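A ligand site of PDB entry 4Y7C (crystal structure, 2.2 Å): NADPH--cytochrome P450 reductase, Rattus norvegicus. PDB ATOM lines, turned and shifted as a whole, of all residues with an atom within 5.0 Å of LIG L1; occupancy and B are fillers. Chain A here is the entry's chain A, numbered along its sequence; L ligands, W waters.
The side-chain hydroxyl of Thr 434 sits at hydrogen-bond distance from the backbone NH of Val 419.
NE of Arg 367 is in hydrogen-bond range of OH of Tyr 421 (3.3 Å).
The guanidinium group (NH1) of Arg 367 lies within hydrogen-bond range of the side-chain amide oxygen (OD1) of Asn 322 (3.0 Å).
The side-chain hydroxyl (OG) of Ser 400 lies within hydrogen-bond range of the side-chain carboxylate (OD2) of Asp 618, at 2.7 Å.
N of Gly 431 lies within hydrogen-bond range of O of Val 419 (2.8 Å).
The backbone carbonyl oxygen of Gly 431 is in hydrogen-bond range of the side-chain hydroxyl of Ser 435, at 2.7 Å.
The backbone carbonyl oxygen of His 262 sits at hydrogen-bond distance from the backbone NH of Arg 457 (2.9 Å).
A ring nitrogen (NE2) of His 262 is in hydrogen-bond range of the side-chain carboxylate of Asp 618.
A nitrogen (N9) of LIG L1 lies close to the indole nitrogen of Trp 620 (3.5 Å).
Residues that only touch LIG L1: His 262, Ala 416, Val 419, Tyr 421, Gly 431, Thr 478 and Ala 481.
Hydrophobic or aromatic side chains within 4 Å of LIG L1: His 262, Tyr 399, Ala 416, Val 417, Val 419, Tyr 421, Val 432, Ala 433, Ala 481 and Trp 620.
Within 4 Å of LIG L1: His 262, Arg 367, Arg 397, Tyr 398, Tyr 399, Ser 400, Cys 415, Ala 416, Val 417, Val 419, Tyr 421, Gly 431, Val 432, Ala 433, Thr 434, Thr 478, Ala 481 and Trp 620.
Water W10 bridges O9 of LIG L1 (2.7 Å) and N of Tyr 398 (3.0 Å).
Water W12 lies within hydrogen-bond range of the side-chain hydroxyl (OG1) of Thr 321 (2.7 Å), an oxygen (O1) of LIG L1 (2.8 Å) and the side-chain amide oxygen (OD1) of Asn 322 (2.8 Å).
Water W9 lies within hydrogen-bond range of the side-chain hydroxyl of Tyr 421, an oxygen (O4) of LIG L1 and the guanidinium group of Arg 367.
Water W6 lies within hydrogen-bond range of the chain-end carboxylate (O) of Ser 621 (2.8 Å) and an oxygen (O10) of LIG L1 (2.8 Å).
Water W11 bridges O5 of LIG L1 (3.1 Å) and OD1 of Asn 322 (3.4 Å).
Water W7 lies within hydrogen-bond range of an oxygen (O10) of LIG L1 (3.2 Å) and the chain-end carboxylate of Ser 621 (3.5 Å).
The backbone NH (N) of Tyr 398 sits at hydrogen-bond distance from an oxygen (O9) of LIG L1 (3.5 Å).
An oxygen (O9) of LIG L1 is in hydrogen-bond range of the backbone carbonyl oxygen of Tyr 398 (2.7 Å).
The backbone NH (N) of Thr 434 lies within hydrogen-bond range of an oxygen (O13) of LIG L1, 2.9 Å away.
An oxygen (O13) of LIG L1 is in hydrogen-bond range of the side-chain hydroxyl of Thr 434 (2.7 Å).
A nitrogen (N7) of LIG L1 sits at hydrogen-bond distance from the backbone carbonyl oxygen of Cys 415, at 2.8 Å.
O14 of LIG L1 sits at hydrogen-bond distance from N of Ala 433 (2.8 Å).
The side-chain hydroxyl (OH) of Tyr 399 is in hydrogen-bond range of an oxygen (O11) of LIG L1 (2.8 Å).
The guanidinium group (NH2) of Arg 367 lies within hydrogen-bond range of an oxygen (O6) of LIG L1 (2.9 Å).
NE of Arg 397 is in salt-bridge range of O14 of LIG L1, 2.9 Å away.
An oxygen (O1) of LIG L1 lies within hydrogen-bond range of the backbone NH (N) of Val 432 (2.9 Å).
N of Ser 400 sits at hydrogen-bond distance from O8 of LIG L1, 3.0 Å away.
N8 of LIG L1 is in hydrogen-bond range of OG of Ser 400 (3.5 Å).
The backbone NH (N) of Val 417 is in hydrogen-bond range of an oxygen (O7) of LIG L1, 3.1 Å away.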
ATOM      1  N   HIS A 262     -16.757   6.143  -4.487  1.00  0.00           N
ATOM      2  CA  HIS A 262     -15.354   6.284  -4.101  1.00  0.00           C
ATOM      3  C   HIS A 262     -14.504   6.500  -5.339  1.00  0.00           C
ATOM      4  O   HIS A 262     -14.824   6.022  -6.425  1.00  0.00           O
ATOM      5  CB  HIS A 262     -14.877   5.046  -3.349  1.00  0.00           C
ATOM      6  CG  HIS A 262     -15.547   4.854  -2.027  1.00  0.00           C
ATOM      7  ND1 HIS A 262     -16.478   3.864  -1.789  1.00  0.00           N
ATOM      8  CD2 HIS A 262     -15.408   5.525  -0.859  1.00  0.00           C
ATOM      9  CE1 HIS A 262     -16.891   3.935  -0.538  1.00  0.00           C
ATOM     10  NE2 HIS A 262     -16.261   4.935   0.052  1.00  0.00           N
ATOM     11  N   THR A 321       6.646   0.059   1.449  1.00  0.00           N
ATOM     12  CA  THR A 321       6.446   0.785   2.696  1.00  0.00           C
ATOM     13  C   THR A 321       5.797  -0.024   3.807  1.00  0.00           C
ATOM     14  O   THR A 321       6.112   0.168   4.970  1.00  0.00           O
ATOM     15  CB  THR A 321       5.604   2.042   2.436  1.00  0.00           C
ATOM     16  OG1 THR A 321       4.485   1.684   1.603  1.00  0.00           O
ATOM     17  CG2 THR A 321       6.432   3.105   1.735  1.00  0.00           C
ATOM     18  N   ASN A 322       4.882  -0.919   3.457  1.00  0.00           N
ATOM     19  CA  ASN A 322       4.258  -1.717   4.501  1.00  0.00           C
ATOM     20  C   ASN A 322       5.219  -2.765   5.038  1.00  0.00           C
ATOM     21  O   ASN A 322       6.138  -3.190   4.343  1.00  0.00           O
ATOM     22  CB  ASN A 322       2.975  -2.380   3.963  1.00  0.00           C
ATOM     23  CG  ASN A 322       1.854  -1.375   3.788  1.00  0.00           C
ATOM     24  OD1 ASN A 322       1.618  -0.538   4.665  1.00  0.00           O
ATOM     25  ND2 ASN A 322       1.155  -1.447   2.654  1.00  0.00           N
ATOM     26  N   ARG A 367       6.615  -0.870  12.573  1.00  0.00           N
ATOM     27  CA  ARG A 367       6.300  -0.475  11.204  1.00  0.00           C
ATOM     28  C   ARG A 367       7.561  -0.295  10.347  1.00  0.00           C
ATOM     29  O   ARG A 367       7.733   0.717   9.669  1.00  0.00           O
ATOM     30  CB  ARG A 367       5.482   0.820  11.197  1.00  0.00           C
ATOM     31  CG  ARG A 367       4.086   0.710  11.800  1.00  0.00           C
ATOM     32  CD  ARG A 367       3.112  -0.016  10.872  1.00  0.00           C
ATOM     33  NE  ARG A 367       3.148   0.499   9.501  1.00  0.00           N
ATOM     34  CZ  ARG A 367       2.343   0.093   8.518  1.00  0.00           C
ATOM     35  NH1 ARG A 367       2.459   0.618   7.310  1.00  0.00           N
ATOM     36  NH2 ARG A 367       1.419  -0.849   8.745  1.00  0.00           N
ATOM     37  N   ARG A 397      -5.395   3.555  -3.716  1.00  0.00           N
ATOM     38  CA  ARG A 397      -6.013   3.992  -2.479  1.00  0.00           C
ATOM     39  C   ARG A 397      -7.394   4.596  -2.797  1.00  0.00           C
ATOM     40  O   ARG A 397      -7.566   5.270  -3.818  1.00  0.00           O
ATOM     41  CB  ARG A 397      -5.138   5.017  -1.773  1.00  0.00           C
ATOM     42  CG  ARG A 397      -4.078   4.439  -0.825  1.00  0.00           C
ATOM     43  CD  ARG A 397      -2.981   3.642  -1.531  1.00  0.00           C
ATOM     44  NE  ARG A 397      -1.877   3.358  -0.603  1.00  0.00           N
ATOM     45  CZ  ARG A 397      -0.926   2.446  -0.799  1.00  0.00           C
ATOM     46  NH1 ARG A 397       0.029   2.284   0.117  1.00  0.00           N
ATOM     47  NH2 ARG A 397      -0.927   1.686  -1.882  1.00  0.00           N
ATOM     48  N   TYR A 398      -8.357   4.342  -1.926  1.00  0.00           N
ATOM     49  CA  TYR A 398      -9.713   4.856  -2.110  1.00  0.00           C
ATOM     50  C   TYR A 398     -10.011   6.084  -1.280  1.00  0.00           C
ATOM     51  O   TYR A 398      -9.528   6.225  -0.157  1.00  0.00           O
ATOM     52  CB  TYR A 398     -10.744   3.767  -1.786  1.00  0.00           C
ATOM     53  CG  TYR A 398     -10.753   2.658  -2.808  1.00  0.00           C
ATOM     54  CD1 TYR A 398     -11.521   2.770  -3.960  1.00  0.00           C
ATOM     55  CD2 TYR A 398      -9.960   1.524  -2.646  1.00  0.00           C
ATOM     56  CE1 TYR A 398     -11.493   1.791  -4.948  1.00  0.00           C
ATOM     57  CE2 TYR A 398      -9.922   0.531  -3.637  1.00  0.00           C
ATOM     58  CZ  TYR A 398     -10.690   0.669  -4.779  1.00  0.00           C
ATOM     59  OH  TYR A 398     -10.668  -0.291  -5.777  1.00  0.00           O
ATOM     60  N   TYR A 399     -10.831   6.975  -1.834  1.00  0.00           N
ATOM     61  CA  TYR A 399     -11.225   8.192  -1.148  1.00  0.00           C
ATOM     62  C   TYR A 399     -12.694   8.424  -1.418  1.00  0.00           C
ATOM     63  O   TYR A 399     -13.184   8.161  -2.520  1.00  0.00           O
ATOM     64  CB  TYR A 399     -10.373   9.370  -1.653  1.00  0.00           C
ATOM     65  CG  TYR A 399      -8.929   9.215  -1.267  1.00  0.00           C
ATOM     66  CD1 TYR A 399      -8.502   9.538   0.020  1.00  0.00           C
ATOM     67  CD2 TYR A 399      -8.012   8.637  -2.135  1.00  0.00           C
ATOM     68  CE1 TYR A 399      -7.196   9.287   0.430  1.00  0.00           C
ATOM     69  CE2 TYR A 399      -6.696   8.372  -1.729  1.00  0.00           C
ATOM     70  CZ  TYR A 399      -6.298   8.698  -0.448  1.00  0.00           C
ATOM     71  OH  TYR A 399      -5.035   8.378  -0.013  1.00  0.00           O
ATOM     72  N   SER A 400     -13.427   8.883  -0.410  1.00  0.00           N
ATOM     73  CA  SER A 400     -14.846   9.132  -0.568  1.00  0.00           C
ATOM     74  C   SER A 400     -15.004  10.432  -1.343  1.00  0.00           C
ATOM     75  O   SER A 400     -14.657  11.503  -0.841  1.00  0.00           O
ATOM     76  CB  SER A 400     -15.496   9.250   0.813  1.00  0.00           C
ATOM     77  OG  SER A 400     -15.269   8.072   1.564  1.00  0.00           O
ATOM     78  N   CYS A 415     -11.071  14.718  -0.086  1.00  0.00           N
ATOM     79  CA  CYS A 415     -10.809  15.297   1.233  1.00  0.00           C
ATOM     80  C   CYS A 415      -9.976  14.239   1.945  1.00  0.00           C
ATOM     81  O   CYS A 415     -10.477  13.143   2.233  1.00  0.00           O
ATOM     82  CB  CYS A 415     -12.119  15.540   1.997  1.00  0.00           C
ATOM     83  SG  CYS A 415     -11.872  15.992   3.730  1.00  0.00           S
ATOM     84  N   ALA A 416      -8.719  14.553   2.229  1.00  0.00           N
ATOM     85  CA  ALA A 416      -7.841  13.584   2.862  1.00  0.00           C
ATOM     86  C   ALA A 416      -6.851  14.143   3.870  1.00  0.00           C
ATOM     87  O   ALA A 416      -6.388  15.284   3.745  1.00  0.00           O
ATOM     88  CB  ALA A 416      -7.096  12.817   1.787  1.00  0.00           C
ATOM     89  N   VAL A 417      -6.511  13.320   4.852  1.00  0.00           N
ATOM     90  CA  VAL A 417      -5.523  13.731   5.851  1.00  0.00           C
ATOM     91  C   VAL A 417      -4.191  13.105   5.437  1.00  0.00           C
ATOM     92  O   VAL A 417      -4.118  11.917   5.133  1.00  0.00           O
ATOM     93  CB  VAL A 417      -5.935  13.284   7.288  1.00  0.00           C
ATOM     94  CG1 VAL A 417      -6.097  11.775   7.363  1.00  0.00           C
ATOM     95  CG2 VAL A 417      -4.883  13.755   8.302  1.00  0.00           C
ATOM     96  N   VAL A 419      -0.818  11.384   5.728  1.00  0.00           N
ATOM     97  CA  VAL A 419      -0.264  10.456   6.715  1.00  0.00           C
ATOM     98  C   VAL A 419       1.237  10.672   6.859  1.00  0.00           C
ATOM     99  O   VAL A 419       1.979  10.643   5.875  1.00  0.00           O
ATOM    100  CB  VAL A 419      -0.533   8.989   6.331  1.00  0.00           C
ATOM    101  CG1 VAL A 419       0.128   8.062   7.345  1.00  0.00           C
ATOM    102  CG2 VAL A 419      -2.030   8.731   6.296  1.00  0.00           C
ATOM    103  N   TYR A 421       3.936   9.944  10.349  1.00  0.00           N
ATOM    104  CA  TYR A 421       4.060   9.673  11.765  1.00  0.00           C
ATOM    105  C   TYR A 421       5.398   9.096  12.153  1.00  0.00           C
ATOM    106  O   TYR A 421       6.117   8.535  11.312  1.00  0.00           O
ATOM    107  CB  TYR A 421       2.975   8.691  12.209  1.00  0.00           C
ATOM    108  CG  TYR A 421       3.055   7.365  11.491  1.00  0.00           C
ATOM    109  CD1 TYR A 421       2.499   7.207  10.219  1.00  0.00           C
ATOM    110  CD2 TYR A 421       3.740   6.284  12.057  1.00  0.00           C
ATOM    111  CE1 TYR A 421       2.618   5.994   9.522  1.00  0.00           C
ATOM    112  CE2 TYR A 421       3.869   5.069  11.362  1.00  0.00           C
ATOM    113  CZ  TYR A 421       3.303   4.938  10.098  1.00  0.00           C
ATOM    114  OH  TYR A 421       3.444   3.758   9.410  1.00  0.00           O
ATOM    115  N   LYS A 430       5.951   7.935   5.895  1.00  0.00           N
ATOM    116  CA  LYS A 430       5.086   8.780   5.087  1.00  0.00           C
ATOM    117  C   LYS A 430       4.051   7.938   4.349  1.00  0.00           C
ATOM    118  O   LYS A 430       4.377   6.897   3.782  1.00  0.00           O
ATOM    119  CB  LYS A 430       5.919   9.545   4.059  1.00  0.00           C
ATOM    120  CG  LYS A 430       7.006  10.430   4.663  1.00  0.00           C
ATOM    121  CD  LYS A 430       6.406  11.659   5.312  1.00  0.00           C
ATOM    122  CE  LYS A 430       5.773  12.571   4.253  1.00  0.00           C
ATOM    123  NZ  LYS A 430       6.801  13.032   3.274  1.00  0.00           N
ATOM    124  N   GLY A 431       2.808   8.410   4.348  1.00  0.00           N
ATOM    125  CA  GLY A 431       1.751   7.708   3.641  1.00  0.00           C
ATOM    126  C   GLY A 431       2.025   7.828   2.157  1.00  0.00           C
ATOM    127  O   GLY A 431       2.245   8.922   1.637  1.00  0.00           O
ATOM    128  N   VAL A 432       2.018   6.699   1.468  1.00  0.00           N
ATOM    129  CA  VAL A 432       2.307   6.675   0.042  1.00  0.00           C
ATOM    130  C   VAL A 432       1.426   7.583  -0.808  1.00  0.00           C
ATOM    131  O   VAL A 432       1.921   8.500  -1.459  1.00  0.00           O
ATOM    132  CB  VAL A 432       2.184   5.254  -0.530  1.00  0.00           C
ATOM    133  CG1 VAL A 432       2.474   5.283  -2.036  1.00  0.00           C
ATOM    134  CG2 VAL A 432       3.137   4.314   0.202  1.00  0.00           C
ATOM    135  N   ALA A 433       0.125   7.300  -0.812  1.00  0.00           N
ATOM    136  CA  ALA A 433      -0.807   8.063  -1.636  1.00  0.00           C
ATOM    137  C   ALA A 433      -1.003   9.512  -1.194  1.00  0.00           C
ATOM    138  O   ALA A 433      -1.057  10.408  -2.032  1.00  0.00           O
ATOM    139  CB  ALA A 433      -2.160   7.352  -1.705  1.00  0.00           C
ATOM    140  N   THR A 434      -1.100   9.753   0.105  1.00  0.00           N
ATOM    141  CA  THR A 434      -1.307  11.121   0.560  1.00  0.00           C
ATOM    142  C   THR A 434      -0.071  11.999   0.377  1.00  0.00           C
ATOM    143  O   THR A 434      -0.190  13.178   0.055  1.00  0.00           O
ATOM    144  CB  THR A 434      -1.798  11.170   2.032  1.00  0.00           C
ATOM    145  OG1 THR A 434      -0.884  10.449   2.867  1.00  0.00           O
ATOM    146  CG2 THR A 434      -3.189  10.548   2.149  1.00  0.00           C
ATOM    147  N   SER A 435       1.127  11.450   0.564  1.00  0.00           N
ATOM    148  CA  SER A 435       2.329  12.261   0.363  1.00  0.00           C
ATOM    149  C   SER A 435       2.373  12.654  -1.106  1.00  0.00           C
ATOM    150  O   SER A 435       2.687  13.789  -1.463  1.00  0.00           O
ATOM    151  CB  SER A 435       3.602  11.485   0.722  1.00  0.00           C
ATOM    152  OG  SER A 435       3.668  11.216   2.116  1.00  0.00           O
ATOM    153  N   ARG A 457     -15.349   3.813  -8.296  1.00  0.00           N
ATOM    154  CA  ARG A 457     -15.952   2.554  -7.893  1.00  0.00           C
ATOM    155  C   ARG A 457     -17.287   2.899  -7.259  1.00  0.00           C
ATOM    156  O   ARG A 457     -17.345   3.611  -6.263  1.00  0.00           O
ATOM    157  CB  ARG A 457     -15.101   1.807  -6.866  1.00  0.00           C
ATOM    158  CG  ARG A 457     -15.698   0.445  -6.492  1.00  0.00           C
ATOM    159  CD  ARG A 457     -14.880  -0.286  -5.445  1.00  0.00           C
ATOM    160  NE  ARG A 457     -14.844   0.466  -4.185  1.00  0.00           N
ATOM    161  CZ  ARG A 457     -14.086   0.132  -3.143  1.00  0.00           C
ATOM    162  NH1 ARG A 457     -13.296  -0.938  -3.189  1.00  0.00           N
ATOM    163  NH2 ARG A 457     -14.124   0.867  -2.031  1.00  0.00           N
ATOM    164  N   THR A 478     -12.176  13.494   8.768  1.00  0.00           N
ATOM    165  CA  THR A 478     -12.289  13.316   7.318  1.00  0.00           C
ATOM    166  C   THR A 478     -13.570  12.565   6.933  1.00  0.00           C
ATOM    167  O   THR A 478     -13.850  12.394   5.755  1.00  0.00           O
ATOM    168  CB  THR A 478     -11.085  12.554   6.713  1.00  0.00           C
ATOM    169  OG1 THR A 478     -10.832  11.368   7.484  1.00  0.00           O
ATOM    170  CG2 THR A 478      -9.856  13.439   6.671  1.00  0.00           C
ATOM    171  N   ALA A 481     -16.174  13.853   4.312  1.00  0.00           N
ATOM    172  CA  ALA A 481     -15.920  13.937   2.864  1.00  0.00           C
ATOM    173  C   ALA A 481     -17.062  13.580   1.894  1.00  0.00           C
ATOM    174  O   ALA A 481     -17.283  14.327   0.944  1.00  0.00           O
ATOM    175  CB  ALA A 481     -14.673  13.126   2.522  1.00  0.00           C
ATOM    176  N   ASP A 618     -19.749   4.248   5.778  1.00  0.00           N
ATOM    177  CA  ASP A 618     -18.637   4.481   4.873  1.00  0.00           C
ATOM    178  C   ASP A 618     -17.470   4.734   5.818  1.00  0.00           C
ATOM    179  O   ASP A 618     -16.967   5.850   5.933  1.00  0.00           O
ATOM    180  CB  ASP A 618     -18.894   5.722   3.999  1.00  0.00           C
ATOM    181  CG  ASP A 618     -17.712   6.043   3.098  1.00  0.00           C
ATOM    182  OD1 ASP A 618     -16.950   5.120   2.766  1.00  0.00           O
ATOM    183  OD2 ASP A 618     -17.550   7.226   2.706  1.00  0.00           O
ATOM    184  N   TRP A 620     -13.602   3.414   7.604  1.00  0.00           N
ATOM    185  CA  TRP A 620     -12.321   2.801   7.298  1.00  0.00           C
ATOM    186  C   TRP A 620     -11.384   3.038   8.459  1.00  0.00           C
ATOM    187  O   TRP A 620     -11.684   3.825   9.371  1.00  0.00           O
ATOM    188  CB  TRP A 620     -11.748   3.414   6.010  1.00  0.00           C
ATOM    189  CG  TRP A 620     -11.438   4.887   6.096  1.00  0.00           C
ATOM    190  CD1 TRP A 620     -10.282   5.462   6.555  1.00  0.00           C
ATOM    191  CD2 TRP A 620     -12.310   5.980   5.752  1.00  0.00           C
ATOM    192  NE1 TRP A 620     -10.378   6.840   6.522  1.00  0.00           N
ATOM    193  CE2 TRP A 620     -11.618   7.178   6.037  1.00  0.00           C
ATOM    194  CE3 TRP A 620     -13.614   6.052   5.237  1.00  0.00           C
ATOM    195  CZ2 TRP A 620     -12.182   8.447   5.826  1.00  0.00           C
ATOM    196  CZ3 TRP A 620     -14.177   7.320   5.026  1.00  0.00           C
ATOM    197  CH2 TRP A 620     -13.458   8.493   5.316  1.00  0.00           C
ATOM    198  N   SER A 621     -10.240   2.365   8.439  1.00  0.00           N
ATOM    199  CA  SER A 621      -9.253   2.493   9.502  1.00  0.00           C
ATOM    200  C   SER A 621      -7.939   3.066   8.983  1.00  0.00           C
ATOM    201  O   SER A 621      -7.823   3.238   7.751  1.00  0.00           O
ATOM    202  CB  SER A 621      -9.000   1.121  10.125  1.00  0.00           C
ATOM    203  OG  SER A 621     -10.224   0.490  10.473  1.00  0.00           O
ATOM    204  OXT SER A 621      -7.036   3.322   9.818  1.00  0.00           O
HETATM  205  P1  LIG L   1      -0.195   4.225   3.456  1.00  0.00           P
HETATM  206  O1  LIG L   1       1.168   4.310   2.905  1.00  0.00           O
HETATM  207  O2  LIG L   1      -1.196   3.354   2.792  1.00  0.00           O
HETATM  208  O3  LIG L   1      -0.102   3.820   5.007  1.00  0.00           O
HETATM  209  C1  LIG L   1      -1.282   3.494   5.744  1.00  0.00           C
HETATM  210  C2  LIG L   1      -0.881   2.754   7.020  1.00  0.00           C
HETATM  211  O4  LIG L   1      -0.008   3.558   7.829  1.00  0.00           O
HETATM  212  C3  LIG L   1      -2.073   2.564   7.937  1.00  0.00           C
HETATM  213  O5  LIG L   1      -2.857   1.461   7.448  1.00  0.00           O
HETATM  214  C4  LIG L   1      -1.325   2.130   9.180  1.00  0.00           C
HETATM  215  O6  LIG L   1      -0.954   0.747   9.069  1.00  0.00           O
HETATM  216  C5  LIG L   1      -0.091   3.014   9.161  1.00  0.00           C
HETATM  217  N1  LIG L   1      -0.237   4.179  10.067  1.00  0.00           N
HETATM  218  C6  LIG L   1      -0.981   5.424   9.772  1.00  0.00           C
HETATM  219  N2  LIG L   1      -0.698   6.200  10.992  1.00  0.00           N
HETATM  220  C7  LIG L   1       0.040   5.455  11.822  1.00  0.00           C
HETATM  221  C8  LIG L   1       0.514   5.751  13.016  1.00  0.00           C
HETATM  222  N3  LIG L   1       0.237   6.959  13.480  1.00  0.00           N
HETATM  223  N4  LIG L   1       1.179   4.855  13.772  1.00  0.00           N
HETATM  224  C9  LIG L   1       1.360   3.567  13.286  1.00  0.00           C
HETATM  225  N5  LIG L   1       0.829   3.275  12.024  1.00  0.00           N
HETATM  226  C10 LIG L   1       0.189   4.220  11.317  1.00  0.00           C
HETATM  227  N6  LIG L   1      -8.835   8.650   3.758  1.00  0.00           N
HETATM  228  C11 LIG L   1      -9.048  10.027   3.696  1.00  0.00           C
HETATM  229  O7  LIG L   1      -8.229  10.793   4.191  1.00  0.00           O
HETATM  230  N7  LIG L   1     -10.224  10.525   3.124  1.00  0.00           N
HETATM  231  C12 LIG L   1     -11.191   9.633   2.632  1.00  0.00           C
HETATM  232  O8  LIG L   1     -12.200  10.084   2.075  1.00  0.00           O
HETATM  233  C13 LIG L   1     -10.978   8.260   2.702  1.00  0.00           C
HETATM  234  N8  LIG L   1     -11.966   7.415   2.385  1.00  0.00           N
HETATM  235  C14 LIG L   1     -11.753   6.098   2.430  1.00  0.00           C
HETATM  236  C15 LIG L   1     -12.743   5.218   2.006  1.00  0.00           C
HETATM  237  C16 LIG L   1     -12.499   3.852   1.979  1.00  0.00           C
HETATM  238  C17 LIG L   1     -13.428   2.987   1.413  1.00  0.00           C
HETATM  239  C18 LIG L   1     -11.263   3.355   2.403  1.00  0.00           C
HETATM  240  C19 LIG L   1     -11.014   1.987   2.399  1.00  0.00           C
HETATM  241  C20 LIG L   1     -10.272   4.231   2.818  1.00  0.00           C
HETATM  242  C21 LIG L   1     -10.509   5.607   2.820  1.00  0.00           C
HETATM  243  N9  LIG L   1      -9.526   6.464   3.164  1.00  0.00           N
HETATM  244  C22 LIG L   1      -9.810   7.768   3.259  1.00  0.00           C
HETATM  245  C23 LIG L   1      -8.192   5.973   3.568  1.00  0.00           C
HETATM  246  C24 LIG L   1      -7.271   5.916   2.345  1.00  0.00           C
HETATM  247  O9  LIG L   1      -7.761   4.937   1.432  1.00  0.00           O
HETATM  248  C25 LIG L   1      -5.829   5.567   2.743  1.00  0.00           C
HETATM  249  O10 LIG L   1      -5.818   4.384   3.541  1.00  0.00           O
HETATM  250  C26 LIG L   1      -5.211   6.730   3.524  1.00  0.00           C
HETATM  251  O11 LIG L   1      -5.343   7.948   2.779  1.00  0.00           O
HETATM  252  C27 LIG L   1      -3.728   6.429   3.795  1.00  0.00           C
HETATM  253  O12 LIG L   1      -3.106   6.036   2.559  1.00  0.00           O
HETATM  254  P2  LIG L   1      -1.564   6.374   2.264  1.00  0.00           P
HETATM  255  O13 LIG L   1      -1.362   7.832   2.318  1.00  0.00           O
HETATM  256  O14 LIG L   1      -1.174   5.643   1.038  1.00  0.00           O
HETATM  257  O15 LIG L   1      -0.803   5.714   3.526  1.00  0.00           O
HETATM  258  N1  LG2 L   2     -14.016  -7.768   7.155  1.00  0.00           N
HETATM  259  C1  LG2 L   2     -15.070  -8.486   7.582  1.00  0.00           C
HETATM  260  O1  LG2 L   2     -14.930  -9.517   8.228  1.00  0.00           O
HETATM  261  N2  LG2 L   2     -16.318  -7.998   7.260  1.00  0.00           N
HETATM  262  C2  LG2 L   2     -16.624  -6.836   6.537  1.00  0.00           C
HETATM  263  O2  LG2 L   2     -17.822  -6.617   6.382  1.00  0.00           O
HETATM  264  C3  LG2 L   2     -15.509  -6.060   6.093  1.00  0.00           C
HETATM  265  N3  LG2 L   2     -15.779  -4.864   5.361  1.00  0.00           N
HETATM  266  C4  LG2 L   2     -14.622  -4.171   4.973  1.00  0.00           C
HETATM  267  C5  LG2 L   2     -14.859  -2.948   4.244  1.00  0.00           C
HETATM  268  C6  LG2 L   2     -13.779  -2.136   3.789  1.00  0.00           C
HETATM  269  C7  LG2 L   2     -14.175  -0.842   3.024  1.00  0.00           C
HETATM  270  C8  LG2 L   2     -12.358  -2.535   4.062  1.00  0.00           C
HETATM  271  C9  LG2 L   2     -11.232  -1.834   3.677  1.00  0.00           C
HETATM  272  C10 LG2 L   2     -12.130  -3.715   4.759  1.00  0.00           C
HETATM  273  C11 LG2 L   2     -13.229  -4.558   5.237  1.00  0.00           C
HETATM  274  N4  LG2 L   2     -13.051  -5.817   5.985  1.00  0.00           N
HETATM  275  C12 LG2 L   2     -14.218  -6.593   6.432  1.00  0.00           C
HETATM  276  C13 LG2 L   2     -11.706  -6.300   6.286  1.00  0.00           C
HETATM  277  C14 LG2 L   2     -11.102  -7.181   5.141  1.00  0.00           C
HETATM  278  O3  LG2 L   2     -11.966  -8.372   4.949  1.00  0.00           O
HETATM  279  C15 LG2 L   2      -9.706  -7.632   5.513  1.00  0.00           C
HETATM  280  O4  LG2 L   2      -8.907  -6.429   5.679  1.00  0.00           O
HETATM  281  C16 LG2 L   2      -9.116  -8.543   4.370  1.00  0.00           C
HETATM  282  O5  LG2 L   2      -7.820  -8.877   4.939  1.00  0.00           O
HETATM  283  C17 LG2 L   2      -8.805  -7.819   3.067  1.00  0.00           C
HETATM  284  O6  LG2 L   2      -8.259  -8.741   2.033  1.00  0.00           O
HETATM  285  P1  LG2 L   2      -7.777  -8.362   0.572  1.00  0.00           P
HETATM  286  O7  LG2 L   2      -6.571  -7.522   0.670  1.00  0.00           O
HETATM  287  O8  LG2 L   2      -9.061  -7.806  -0.143  1.00  0.00           O
HETATM  288  O9  LG2 L   2      -7.352  -9.805   0.018  1.00  0.00           O
HETATM  289  O   HOH W   1      -3.827   2.824   2.596  1.00  0.00           O
HETATM  290  O   HOH W   2     -12.092  12.243   0.239  1.00  0.00           O
HETATM  291  O   HOH W   3      -1.494   8.683  11.382  1.00  0.00           O
HETATM  292  O   HOH W   4       3.880   4.328   4.656  1.00  0.00           O
HETATM  293  O   HOH W   5      -1.063   0.451   2.773  1.00  0.00           O
HETATM  294  O   HOH W   6      -5.627   4.271   6.365  1.00  0.00           O
HETATM  295  O   HOH W   7      -7.934   2.155   4.428  1.00  0.00           O
HETATM  296  O   HOH W   8      -5.838   9.723   4.650  1.00  0.00           O
HETATM  297  O   HOH W   9       2.630   3.603   6.938  1.00  0.00           O
HETATM  298  O   HOH W  10      -7.524   2.511   0.293  1.00  0.00           O
HETATM  299  O   HOH W  11      -1.684  -0.571   5.491  1.00  0.00           O
HETATM  300  O   HOH W  12       2.262   1.776   3.142  1.00  0.00           O
